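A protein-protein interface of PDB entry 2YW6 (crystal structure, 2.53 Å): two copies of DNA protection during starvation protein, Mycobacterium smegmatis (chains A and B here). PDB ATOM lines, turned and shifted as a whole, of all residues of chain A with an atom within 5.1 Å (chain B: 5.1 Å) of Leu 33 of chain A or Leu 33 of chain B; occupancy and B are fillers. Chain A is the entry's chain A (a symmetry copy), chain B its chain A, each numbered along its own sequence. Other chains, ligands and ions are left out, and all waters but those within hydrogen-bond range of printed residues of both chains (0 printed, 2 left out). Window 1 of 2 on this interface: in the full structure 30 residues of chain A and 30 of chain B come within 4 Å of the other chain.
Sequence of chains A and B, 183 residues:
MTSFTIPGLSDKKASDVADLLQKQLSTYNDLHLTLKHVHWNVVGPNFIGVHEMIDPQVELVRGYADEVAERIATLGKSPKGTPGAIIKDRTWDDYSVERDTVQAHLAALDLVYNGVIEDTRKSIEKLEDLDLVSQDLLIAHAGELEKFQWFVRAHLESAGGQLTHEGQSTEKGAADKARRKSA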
ATOM      1  N   TYR A  28      23.186 -27.938 -13.546  1.00  0.00           N
ATOM      2  CA  TYR A  28      23.222 -29.208 -12.824  1.00  0.00           C
ATOM      3  C   TYR A  28      23.194 -29.056 -11.303  1.00  0.00           C
ATOM      4  O   TYR A  28      22.441 -29.762 -10.621  1.00  0.00           O
ATOM      5  CB  TYR A  28      24.457 -30.007 -13.240  1.00  0.00           C
ATOM      6  CG  TYR A  28      24.412 -30.497 -14.677  1.00  0.00           C
ATOM      7  CD1 TYR A  28      25.587 -30.808 -15.365  1.00  0.00           C
ATOM      8  CD2 TYR A  28      23.193 -30.630 -15.356  1.00  0.00           C
ATOM      9  CE1 TYR A  28      25.558 -31.230 -16.680  1.00  0.00           C
ATOM     10  CE2 TYR A  28      23.154 -31.054 -16.675  1.00  0.00           C
ATOM     11  CZ  TYR A  28      24.344 -31.348 -17.334  1.00  0.00           C
ATOM     12  OH  TYR A  28      24.322 -31.727 -18.662  1.00  0.00           O
ATOM     13  N   ASN A  29      24.003 -28.135 -10.772  1.00  0.00           N
ATOM     14  CA  ASN A  29      24.059 -27.907  -9.326  1.00  0.00           C
ATOM     15  C   ASN A  29      22.719 -27.453  -8.777  1.00  0.00           C
ATOM     16  O   ASN A  29      22.239 -27.959  -7.758  1.00  0.00           O
ATOM     17  CB  ASN A  29      25.130 -26.870  -8.977  1.00  0.00           C
ATOM     18  CG  ASN A  29      26.533 -27.385  -9.213  1.00  0.00           C
ATOM     19  OD1 ASN A  29      26.752 -28.595  -9.288  1.00  0.00           O
ATOM     20  ND2 ASN A  29      27.500 -26.471  -9.319  1.00  0.00           N
ATOM     21  N   ASP A  30      22.120 -26.486  -9.458  1.00  0.00           N
ATOM     22  CA  ASP A  30      20.831 -25.971  -9.044  1.00  0.00           C
ATOM     23  C   ASP A  30      19.801 -27.074  -9.221  1.00  0.00           C
ATOM     24  O   ASP A  30      18.820 -27.144  -8.482  1.00  0.00           O
ATOM     25  CB  ASP A  30      20.460 -24.753  -9.883  1.00  0.00           C
ATOM     26  CG  ASP A  30      19.293 -23.992  -9.309  1.00  0.00           C
ATOM     27  OD1 ASP A  30      19.143 -22.798  -9.635  1.00  0.00           O
ATOM     28  OD2 ASP A  30      18.522 -24.582  -8.532  1.00  0.00           O
ATOM     29  N   LEU A  31      20.040 -27.952 -10.193  1.00  0.00           N
ATOM     30  CA  LEU A  31      19.121 -29.051 -10.450  1.00  0.00           C
ATOM     31  C   LEU A  31      19.178 -30.143  -9.371  1.00  0.00           C
ATOM     32  O   LEU A  31      18.132 -30.517  -8.820  1.00  0.00           O
ATOM     33  CB  LEU A  31      19.370 -29.662 -11.840  1.00  0.00           C
ATOM     34  CG  LEU A  31      18.367 -30.752 -12.266  1.00  0.00           C
ATOM     35  CD1 LEU A  31      16.945 -30.215 -12.140  1.00  0.00           C
ATOM     36  CD2 LEU A  31      18.655 -31.229 -13.699  1.00  0.00           C
ATOM     37  N   HIS A  32      20.368 -30.646  -9.041  1.00  0.00           N
ATOM     38  CA  HIS A  32      20.406 -31.689  -8.024  1.00  0.00           C
ATOM     39  C   HIS A  32      20.090 -31.173  -6.632  1.00  0.00           C
ATOM     40  O   HIS A  32      19.782 -31.965  -5.736  1.00  0.00           O
ATOM     41  CB  HIS A  32      21.719 -32.507  -8.056  1.00  0.00           C
ATOM     42  CG  HIS A  32      22.953 -31.748  -7.671  1.00  0.00           C
ATOM     43  ND1 HIS A  32      23.288 -31.471  -6.364  1.00  0.00           N
ATOM     44  CD2 HIS A  32      23.973 -31.279  -8.430  1.00  0.00           C
ATOM     45  CE1 HIS A  32      24.462 -30.868  -6.333  1.00  0.00           C
ATOM     46  NE2 HIS A  32      24.901 -30.740  -7.574  1.00  0.00           N
ATOM     47  N   LEU A  33      20.141 -29.857  -6.440  1.00  0.00           N
ATOM     48  CA  LEU A  33      19.769 -29.313  -5.141  1.00  0.00           C
ATOM     49  C   LEU A  33      18.232 -29.317  -5.132  1.00  0.00           C
ATOM     50  O   LEU A  33      17.585 -29.754  -4.174  1.00  0.00           O
ATOM     51  CB  LEU A  33      20.295 -27.880  -4.947  1.00  0.00           C
ATOM     52  CG  LEU A  33      21.789 -27.624  -4.693  1.00  0.00           C
ATOM     53  CD1 LEU A  33      22.000 -26.131  -4.376  1.00  0.00           C
ATOM     54  CD2 LEU A  33      22.288 -28.488  -3.545  1.00  0.00           C
ATOM     55  N   THR A  34      17.660 -28.849  -6.231  1.00  0.00           N
ATOM     56  CA  THR A  34      16.219 -28.793  -6.376  1.00  0.00           C
ATOM     57  C   THR A  34      15.601 -30.188  -6.351  1.00  0.00           C
ATOM     58  O   THR A  34      14.523 -30.375  -5.784  1.00  0.00           O
ATOM     59  CB  THR A  34      15.851 -28.071  -7.672  1.00  0.00           C
ATOM     60  OG1 THR A  34      16.362 -26.734  -7.618  1.00  0.00           O
ATOM     61  CG2 THR A  34      14.344 -28.044  -7.857  1.00  0.00           C
ATOM     62  N   LEU A  35      16.276 -31.160  -6.961  1.00  0.00           N
ATOM     63  CA  LEU A  35      15.786 -32.536  -6.962  1.00  0.00           C
ATOM     64  C   LEU A  35      15.659 -33.015  -5.503  1.00  0.00           C
ATOM     65  O   LEU A  35      14.668 -33.651  -5.121  1.00  0.00           O
ATOM     66  CB  LEU A  35      16.761 -33.441  -7.727  1.00  0.00           C
ATOM     67  CG  LEU A  35      16.442 -33.999  -9.125  1.00  0.00           C
ATOM     68  CD1 LEU A  35      15.299 -33.260  -9.763  1.00  0.00           C
ATOM     69  CD2 LEU A  35      17.696 -33.918 -10.003  1.00  0.00           C
ATOM     70  N   LYS A  36      16.668 -32.717  -4.691  1.00  0.00           N
ATOM     71  CA  LYS A  36      16.630 -33.109  -3.294  1.00  0.00           C
ATOM     72  C   LYS A  36      15.504 -32.375  -2.569  1.00  0.00           C
ATOM     73  O   LYS A  36      14.764 -32.970  -1.788  1.00  0.00           O
ATOM     74  CB  LYS A  36      17.976 -32.831  -2.630  1.00  0.00           C
ATOM     75  CG  LYS A  36      18.941 -34.002  -2.758  1.00  0.00           C
ATOM     76  CD  LYS A  36      18.315 -35.264  -2.165  1.00  0.00           C
ATOM     77  CE  LYS A  36      19.294 -36.416  -2.104  1.00  0.00           C
ATOM     78  NZ  LYS A  36      18.700 -37.638  -1.468  1.00  0.00           N
ATOM     79  N   HIS A  37      15.377 -31.085  -2.846  1.00  0.00           N
ATOM     80  CA  HIS A  37      14.337 -30.268  -2.248  1.00  0.00           C
ATOM     81  C   HIS A  37      12.932 -30.859  -2.487  1.00  0.00           C
ATOM     82  O   HIS A  37      12.137 -30.952  -1.554  1.00  0.00           O
ATOM     83  CB  HIS A  37      14.408 -28.853  -2.827  1.00  0.00           C
ATOM     84  CG  HIS A  37      13.307 -27.951  -2.360  1.00  0.00           C
ATOM     85  ND1 HIS A  37      13.426 -27.128  -1.260  1.00  0.00           N
ATOM     86  CD2 HIS A  37      12.050 -27.771  -2.831  1.00  0.00           C
ATOM     87  CE1 HIS A  37      12.293 -26.482  -1.071  1.00  0.00           C
ATOM     88  NE2 HIS A  37      11.438 -26.852  -2.012  1.00  0.00           N
ATOM     89  N   GLY A  81      31.556 -23.916  -8.563  1.00  0.00           N
ATOM     90  CA  GLY A  81      30.464 -24.693  -8.008  1.00  0.00           C
ATOM     91  C   GLY A  81      29.852 -24.204  -6.709  1.00  0.00           C
ATOM     92  O   GLY A  81      29.026 -24.897  -6.111  1.00  0.00           O
ATOM     93  N   THR A  82      30.228 -23.013  -6.257  1.00  0.00           N
ATOM     94  CA  THR A  82      29.674 -22.510  -5.006  1.00  0.00           C
ATOM     95  C   THR A  82      28.276 -21.972  -5.223  1.00  0.00           C
ATOM     96  O   THR A  82      27.859 -21.737  -6.352  1.00  0.00           O
ATOM     97  CB  THR A  82      30.544 -21.392  -4.412  1.00  0.00           C
ATOM     98  OG1 THR A  82      30.503 -20.249  -5.272  1.00  0.00           O
ATOM     99  CG2 THR A  82      31.979 -21.859  -4.269  1.00  0.00           C
ATOM    100  N   PRO A  83      27.520 -21.793  -4.132  1.00  0.00           N
ATOM    101  CA  PRO A  83      26.153 -21.270  -4.236  1.00  0.00           C
ATOM    102  C   PRO A  83      26.156 -19.952  -5.011  1.00  0.00           C
ATOM    103  O   PRO A  83      25.286 -19.702  -5.845  1.00  0.00           O
ATOM    104  CB  PRO A  83      25.763 -21.078  -2.774  1.00  0.00           C
ATOM    105  CG  PRO A  83      26.494 -22.199  -2.097  1.00  0.00           C
ATOM    106  CD  PRO A  83      27.851 -22.130  -2.740  1.00  0.00           C
ATOM    107  N   ILE A  86      26.241 -20.361  -8.696  1.00  0.00           N
ATOM    108  CA  ILE A  86      24.929 -20.721  -9.207  1.00  0.00           C
ATOM    109  C   ILE A  86      24.054 -19.493  -9.422  1.00  0.00           C
ATOM    110  O   ILE A  86      23.444 -19.321 -10.488  1.00  0.00           O
ATOM    111  CB  ILE A  86      24.201 -21.668  -8.246  1.00  0.00           C
ATOM    112  CG1 ILE A  86      25.077 -22.886  -7.958  1.00  0.00           C
ATOM    113  CG2 ILE A  86      22.882 -22.096  -8.854  1.00  0.00           C
ATOM    114  CD1 ILE A  86      24.384 -23.929  -7.140  1.00  0.00           C
ATOM    115  N   TYR B  28      25.267 -27.525   5.462  1.00  0.00           N
ATOM    116  CA  TYR B  28      25.645 -28.743   4.749  1.00  0.00           C
ATOM    117  C   TYR B  28      25.624 -28.600   3.226  1.00  0.00           C
ATOM    118  O   TYR B  28      26.566 -29.030   2.548  1.00  0.00           O
ATOM    119  CB  TYR B  28      24.734 -29.897   5.172  1.00  0.00           C
ATOM    120  CG  TYR B  28      24.934 -30.335   6.612  1.00  0.00           C
ATOM    121  CD1 TYR B  28      23.922 -31.006   7.302  1.00  0.00           C
ATOM    122  CD2 TYR B  28      26.129 -30.061   7.290  1.00  0.00           C
ATOM    123  CE1 TYR B  28      24.085 -31.385   8.621  1.00  0.00           C
ATOM    124  CE2 TYR B  28      26.302 -30.441   8.611  1.00  0.00           C
ATOM    125  CZ  TYR B  28      25.271 -31.100   9.275  1.00  0.00           C
ATOM    126  OH  TYR B  28      25.413 -31.442  10.605  1.00  0.00           O
ATOM    127  N   ASN B  29      24.561 -27.995   2.690  1.00  0.00           N
ATOM    128  CA  ASN B  29      24.435 -27.807   1.243  1.00  0.00           C
ATOM    129  C   ASN B  29      25.557 -26.947   0.689  1.00  0.00           C
ATOM    130  O   ASN B  29      26.176 -27.278  -0.327  1.00  0.00           O
ATOM    131  CB  ASN B  29      23.087 -27.175   0.888  1.00  0.00           C
ATOM    132  CG  ASN B  29      21.926 -28.116   1.129  1.00  0.00           C
ATOM    133  OD1 ASN B  29      22.111 -29.330   1.213  1.00  0.00           O
ATOM    134  ND2 ASN B  29      20.715 -27.562   1.229  1.00  0.00           N
ATOM    135  N   ASP B  30      25.810 -25.833   1.363  1.00  0.00           N
ATOM    136  CA  ASP B  30      26.864 -24.932   0.944  1.00  0.00           C
ATOM    137  C   ASP B  30      28.195 -25.641   1.127  1.00  0.00           C
ATOM    138  O   ASP B  30      29.146 -25.395   0.386  1.00  0.00           O
ATOM    139  CB  ASP B  30      26.819 -23.654   1.774  1.00  0.00           C
ATOM    140  CG  ASP B  30      27.677 -22.560   1.193  1.00  0.00           C
ATOM    141  OD1 ASP B  30      27.433 -21.380   1.511  1.00  0.00           O
ATOM    142  OD2 ASP B  30      28.599 -22.874   0.419  1.00  0.00           O
ATOM    143  N   LEU B  31      28.252 -26.543   2.105  1.00  0.00           N
ATOM    144  CA  LEU B  31      29.477 -27.283   2.369  1.00  0.00           C
ATOM    145  C   LEU B  31      29.778 -28.343   1.298  1.00  0.00           C
ATOM    146  O   LEU B  31      30.889 -28.361   0.747  1.00  0.00           O
ATOM    147  CB  LEU B  31      29.438 -27.932   3.764  1.00  0.00           C
ATOM    148  CG  LEU B  31      30.739 -28.636   4.195  1.00  0.00           C
ATOM    149  CD1 LEU B  31      31.910 -27.669   4.064  1.00  0.00           C
ATOM    150  CD2 LEU B  31      30.619 -29.170   5.632  1.00  0.00           C
ATOM    151  N   HIS B  32      28.815 -29.207   0.973  1.00  0.00           N
ATOM    152  CA  HIS B  32      29.117 -30.212  -0.037  1.00  0.00           C
ATOM    153  C   HIS B  32      29.252 -29.631  -1.434  1.00  0.00           C
ATOM    154  O   HIS B  32      29.800 -30.286  -2.325  1.00  0.00           O
ATOM    155  CB  HIS B  32      28.141 -31.411   0.002  1.00  0.00           C
ATOM    156  CG  HIS B  32      26.727 -31.095  -0.387  1.00  0.00           C
ATOM    157  ND1 HIS B  32      26.322 -30.950  -1.695  1.00  0.00           N
ATOM    158  CD2 HIS B  32      25.609 -30.976   0.369  1.00  0.00           C
ATOM    159  CE1 HIS B  32      25.017 -30.760  -1.730  1.00  0.00           C
ATOM    160  NE2 HIS B  32      24.558 -30.773  -0.490  1.00  0.00           N
ATOM    161  N   LEU B  33      28.777 -28.403  -1.634  1.00  0.00           N
ATOM    162  CA  LEU B  33      28.955 -27.777  -2.937  1.00  0.00           C
ATOM    163  C   LEU B  33      30.410 -27.283  -2.949  1.00  0.00           C
ATOM    164  O   LEU B  33      31.164 -27.494  -3.904  1.00  0.00           O
ATOM    165  CB  LEU B  33      27.993 -26.593  -3.141  1.00  0.00           C
ATOM    166  CG  LEU B  33      26.497 -26.836  -3.395  1.00  0.00           C
ATOM    167  CD1 LEU B  33      25.814 -25.494  -3.721  1.00  0.00           C
ATOM    168  CD2 LEU B  33      26.306 -27.823  -4.536  1.00  0.00           C
ATOM    169  N   THR B  34      30.798 -26.648  -1.854  1.00  0.00           N
ATOM    170  CA  THR B  34      32.144 -26.127  -1.710  1.00  0.00           C
ATOM    171  C   THR B  34      33.179 -27.247  -1.727  1.00  0.00           C
ATOM    172  O   THR B  34      34.261 -27.079  -2.294  1.00  0.00           O
ATOM    173  CB  THR B  34      32.256 -25.317  -0.420  1.00  0.00           C
ATOM    174  OG1 THR B  34      31.340 -24.217  -0.483  1.00  0.00           O
ATOM    175  CG2 THR B  34      33.674 -24.802  -0.237  1.00  0.00           C
ATOM    176  N   LEU B  35      32.855 -28.381  -1.109  1.00  0.00           N
ATOM    177  CA  LEU B  35      33.765 -29.525  -1.099  1.00  0.00           C
ATOM    178  C   LEU B  35      34.041 -29.946  -2.555  1.00  0.00           C
ATOM    179  O   LEU B  35      35.186 -30.231  -2.933  1.00  0.00           O
ATOM    180  CB  LEU B  35      33.134 -30.691  -0.327  1.00  0.00           C
ATOM    181  CG  LEU B  35      33.615 -31.107   1.074  1.00  0.00           C
ATOM    182  CD1 LEU B  35      34.456 -30.033   1.706  1.00  0.00           C
ATOM    183  CD2 LEU B  35      32.400 -31.429   1.953  1.00  0.00           C
ATOM    184  N   LYS B  36      32.991 -29.997  -3.369  1.00  0.00           N
ATOM    185  CA  LYS B  36      33.155 -30.366  -4.762  1.00  0.00           C
ATOM    186  C   LYS B  36      33.984 -29.311  -5.493  1.00  0.00           C
ATOM    187  O   LYS B  36      34.878 -29.640  -6.271  1.00  0.00           O
ATOM    188  CB  LYS B  36      31.792 -30.542  -5.426  1.00  0.00           C
ATOM    189  CG  LYS B  36      31.259 -31.962  -5.289  1.00  0.00           C
ATOM    190  CD  LYS B  36      32.260 -32.957  -5.875  1.00  0.00           C
ATOM    191  CE  LYS B  36      31.707 -34.364  -5.927  1.00  0.00           C
ATOM    192  NZ  LYS B  36      32.666 -35.333  -6.555  1.00  0.00           N
ATOM    193  N   HIS B  37      33.686 -28.048  -5.226  1.00  0.00           N
ATOM    194  CA  HIS B  37      34.407 -26.942  -5.830  1.00  0.00           C
ATOM    195  C   HIS B  37      35.927 -27.045  -5.589  1.00  0.00           C
ATOM    196  O   HIS B  37      36.710 -26.882  -6.522  1.00  0.00           O
ATOM    197  CB  HIS B  37      33.880 -25.622  -5.261  1.00  0.00           C
ATOM    198  CG  HIS B  37      34.631 -24.415  -5.735  1.00  0.00           C
ATOM    199  ND1 HIS B  37      34.253 -23.683  -6.841  1.00  0.00           N
ATOM    200  CD2 HIS B  37      35.762 -23.834  -5.267  1.00  0.00           C
ATOM    201  CE1 HIS B  37      35.115 -22.705  -7.036  1.00  0.00           C
ATOM    202  NE2 HIS B  37      36.043 -22.773  -6.094  1.00  0.00           N
ATOM    203  N   GLY B  81      16.051 -26.464   0.460  1.00  0.00           N
ATOM    204  CA  GLY B  81      17.336 -26.849  -0.090  1.00  0.00           C
ATOM    205  C   GLY B  81      17.758 -26.197  -1.394  1.00  0.00           C
ATOM    206  O   GLY B  81      18.765 -26.590  -1.987  1.00  0.00           O
ATOM    207  N   THR B  82      17.018 -25.194  -1.852  1.00  0.00           N
ATOM    208  CA  THR B  82      17.380 -24.549  -3.108  1.00  0.00           C
ATOM    209  C   THR B  82      18.529 -23.585  -2.896  1.00  0.00           C
ATOM    210  O   THR B  82      18.846 -23.220  -1.770  1.00  0.00           O
ATOM    211  CB  THR B  82      16.196 -23.777  -3.709  1.00  0.00           C
ATOM    212  OG1 THR B  82      15.864 -22.675  -2.856  1.00  0.00           O
ATOM    213  CG2 THR B  82      14.990 -24.684  -3.847  1.00  0.00           C
ATOM    214  N   PRO B  83      19.188 -23.179  -3.989  1.00  0.00           N
ATOM    215  CA  PRO B  83      20.311 -22.241  -3.891  1.00  0.00           C
ATOM    216  C   PRO B  83      19.880 -20.989  -3.125  1.00  0.00           C
ATOM    217  O   PRO B  83      20.622 -20.465  -2.293  1.00  0.00           O
ATOM    218  CB  PRO B  83      20.620 -21.943  -5.354  1.00  0.00           C
ATOM    219  CG  PRO B  83      20.292 -23.244  -6.022  1.00  0.00           C
ATOM    220  CD  PRO B  83      18.985 -23.615  -5.379  1.00  0.00           C
ATOM    221  N   ILE B  86      19.929 -21.378   0.564  1.00  0.00           N
ATOM    222  CA  ILE B  86      21.286 -21.291   1.076  1.00  0.00           C
ATOM    223  C   ILE B  86      21.716 -19.844   1.281  1.00  0.00           C
ATOM    224  O   ILE B  86      22.237 -19.477   2.345  1.00  0.00           O
ATOM    225  CB  ILE B  86      22.283 -21.957   0.120  1.00  0.00           C
ATOM    226  CG1 ILE B  86      21.848 -23.396  -0.159  1.00  0.00           C
ATOM    227  CG2 ILE B  86      23.668 -21.931   0.729  1.00  0.00           C
ATOM    228  CD1 ILE B  86      22.842 -24.164  -0.971  1.00  0.00           C
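ND1 of His 37 of chain A is in hydrogen-bond range of N of Gly 81 of chain B (3.2 Å). ND1 of His 37 of chain B lies within hydrogen-bond range of N of Gly 81 of chain A, at 3.2 Å.
The backbone carbonyl oxygen (O) of Asp 30 of chain B lies within hydrogen-bond range of the side-chain hydroxyl (OG1) of Thr 34 of chain B (2.6 Å). The side-chain amide oxygen of Asn 29 of chain A sits at hydrogen-bond distance from a ring nitrogen (NE2) of His 32 of chain A, at 3.3 Å. The backbone carbonyl oxygen (O) of Asp 30 of chain A lies within hydrogen-bond range of the side-chain hydroxyl (OG1) of Thr 34 of chain A (2.6 Å). OD1 of Asn 29 of chain B is in hydrogen-bond range of NE2 of His 32 of chain B (3.3 Å).
Among the printed residues, merely in contact across the chains: Asp 30 of chain A with Pro 83 of chain B, His 32 of chain A with Leu 33 of chain B, Leu 33 of chain A with His 32 of chain B, Leu 33 of chain A with Leu 33 of chain B, Leu 33 of chain A with Gly 81 of chain B, Leu 33 of chain A with Pro 83 of chain B, His 37 of chain A with Thr 82 of chain B, Gly 81 of chain A with Leu 33 of chain B, Thr 82 of chain A with His 37 of chain B, Pro 83 of chain A with Asp 30 of chain B and Pro 83 of chain A with Leu 33 of chain B.
Of the printed residues of chain B, Leu 33 of chain A touches His 32 (3.99 Å), Leu 33 (3.9 Å), Gly 81 (3.6 Å) and Pro 83 (3.7 Å). Of the printed residues of chain B, Gly 81 of chain A touches Leu 33 (3.6 Å) and His 37 (3.2 Å). Of the printed residues of chain B, Thr 82 of chain A touches His 37. Printed residues of chain A within 4 Å of Leu 33 of chain B: His 32 (3.99 Å), Leu 33 (3.9 Å), Gly 81 (3.6 Å) and Pro 83 (3.7 Å). Of the printed residues of chain A, His 37 of chain B touches Gly 81 and Thr 82. The nearest printed residue of chain B that does not touch His 37 of chain A is Pro 83 of chain B (7.4 Å).
Hydrophobic or aromatic side chains of chain B within 4 Å of the printed part of chain A: His 32, Leu 33, His 37 and Pro 83. Printed residues of chain A that touch a printed residue of chain B: Asp 30, His 32, Leu 33, His 37, Gly 81, Thr 82 and Pro 83. Hydrophobic or aromatic side chains of chain A that line the printed part of chain B: His 32, Leu 33, His 37 and Pro 83.
Asp 30 of chain A touches Pro 83 of chain B, and with the chains exchanged Pro 83 of chain A touches Asp 30 of chain B. Leu 33 of chain B touches its own counterpart, Leu 33 of chain A. Leu 33 of chain A touches Pro 83 of chain B, and with the chains exchanged Pro 83 of chain A touches Leu 33 of chain B. His 37 of chain A touches Thr 82 of chain B, and with the chains exchanged Thr 82 of chain A touches His 37 of chain B. Positions printed for both chains: 28, 29, 30, 31, 32, 33, 34, 35, 36, 37, 81, 82, 83 and 86. Of the 13 pairs that touch across the chains among the printed residues, 13 have their exchanged pair printed and touching as well.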
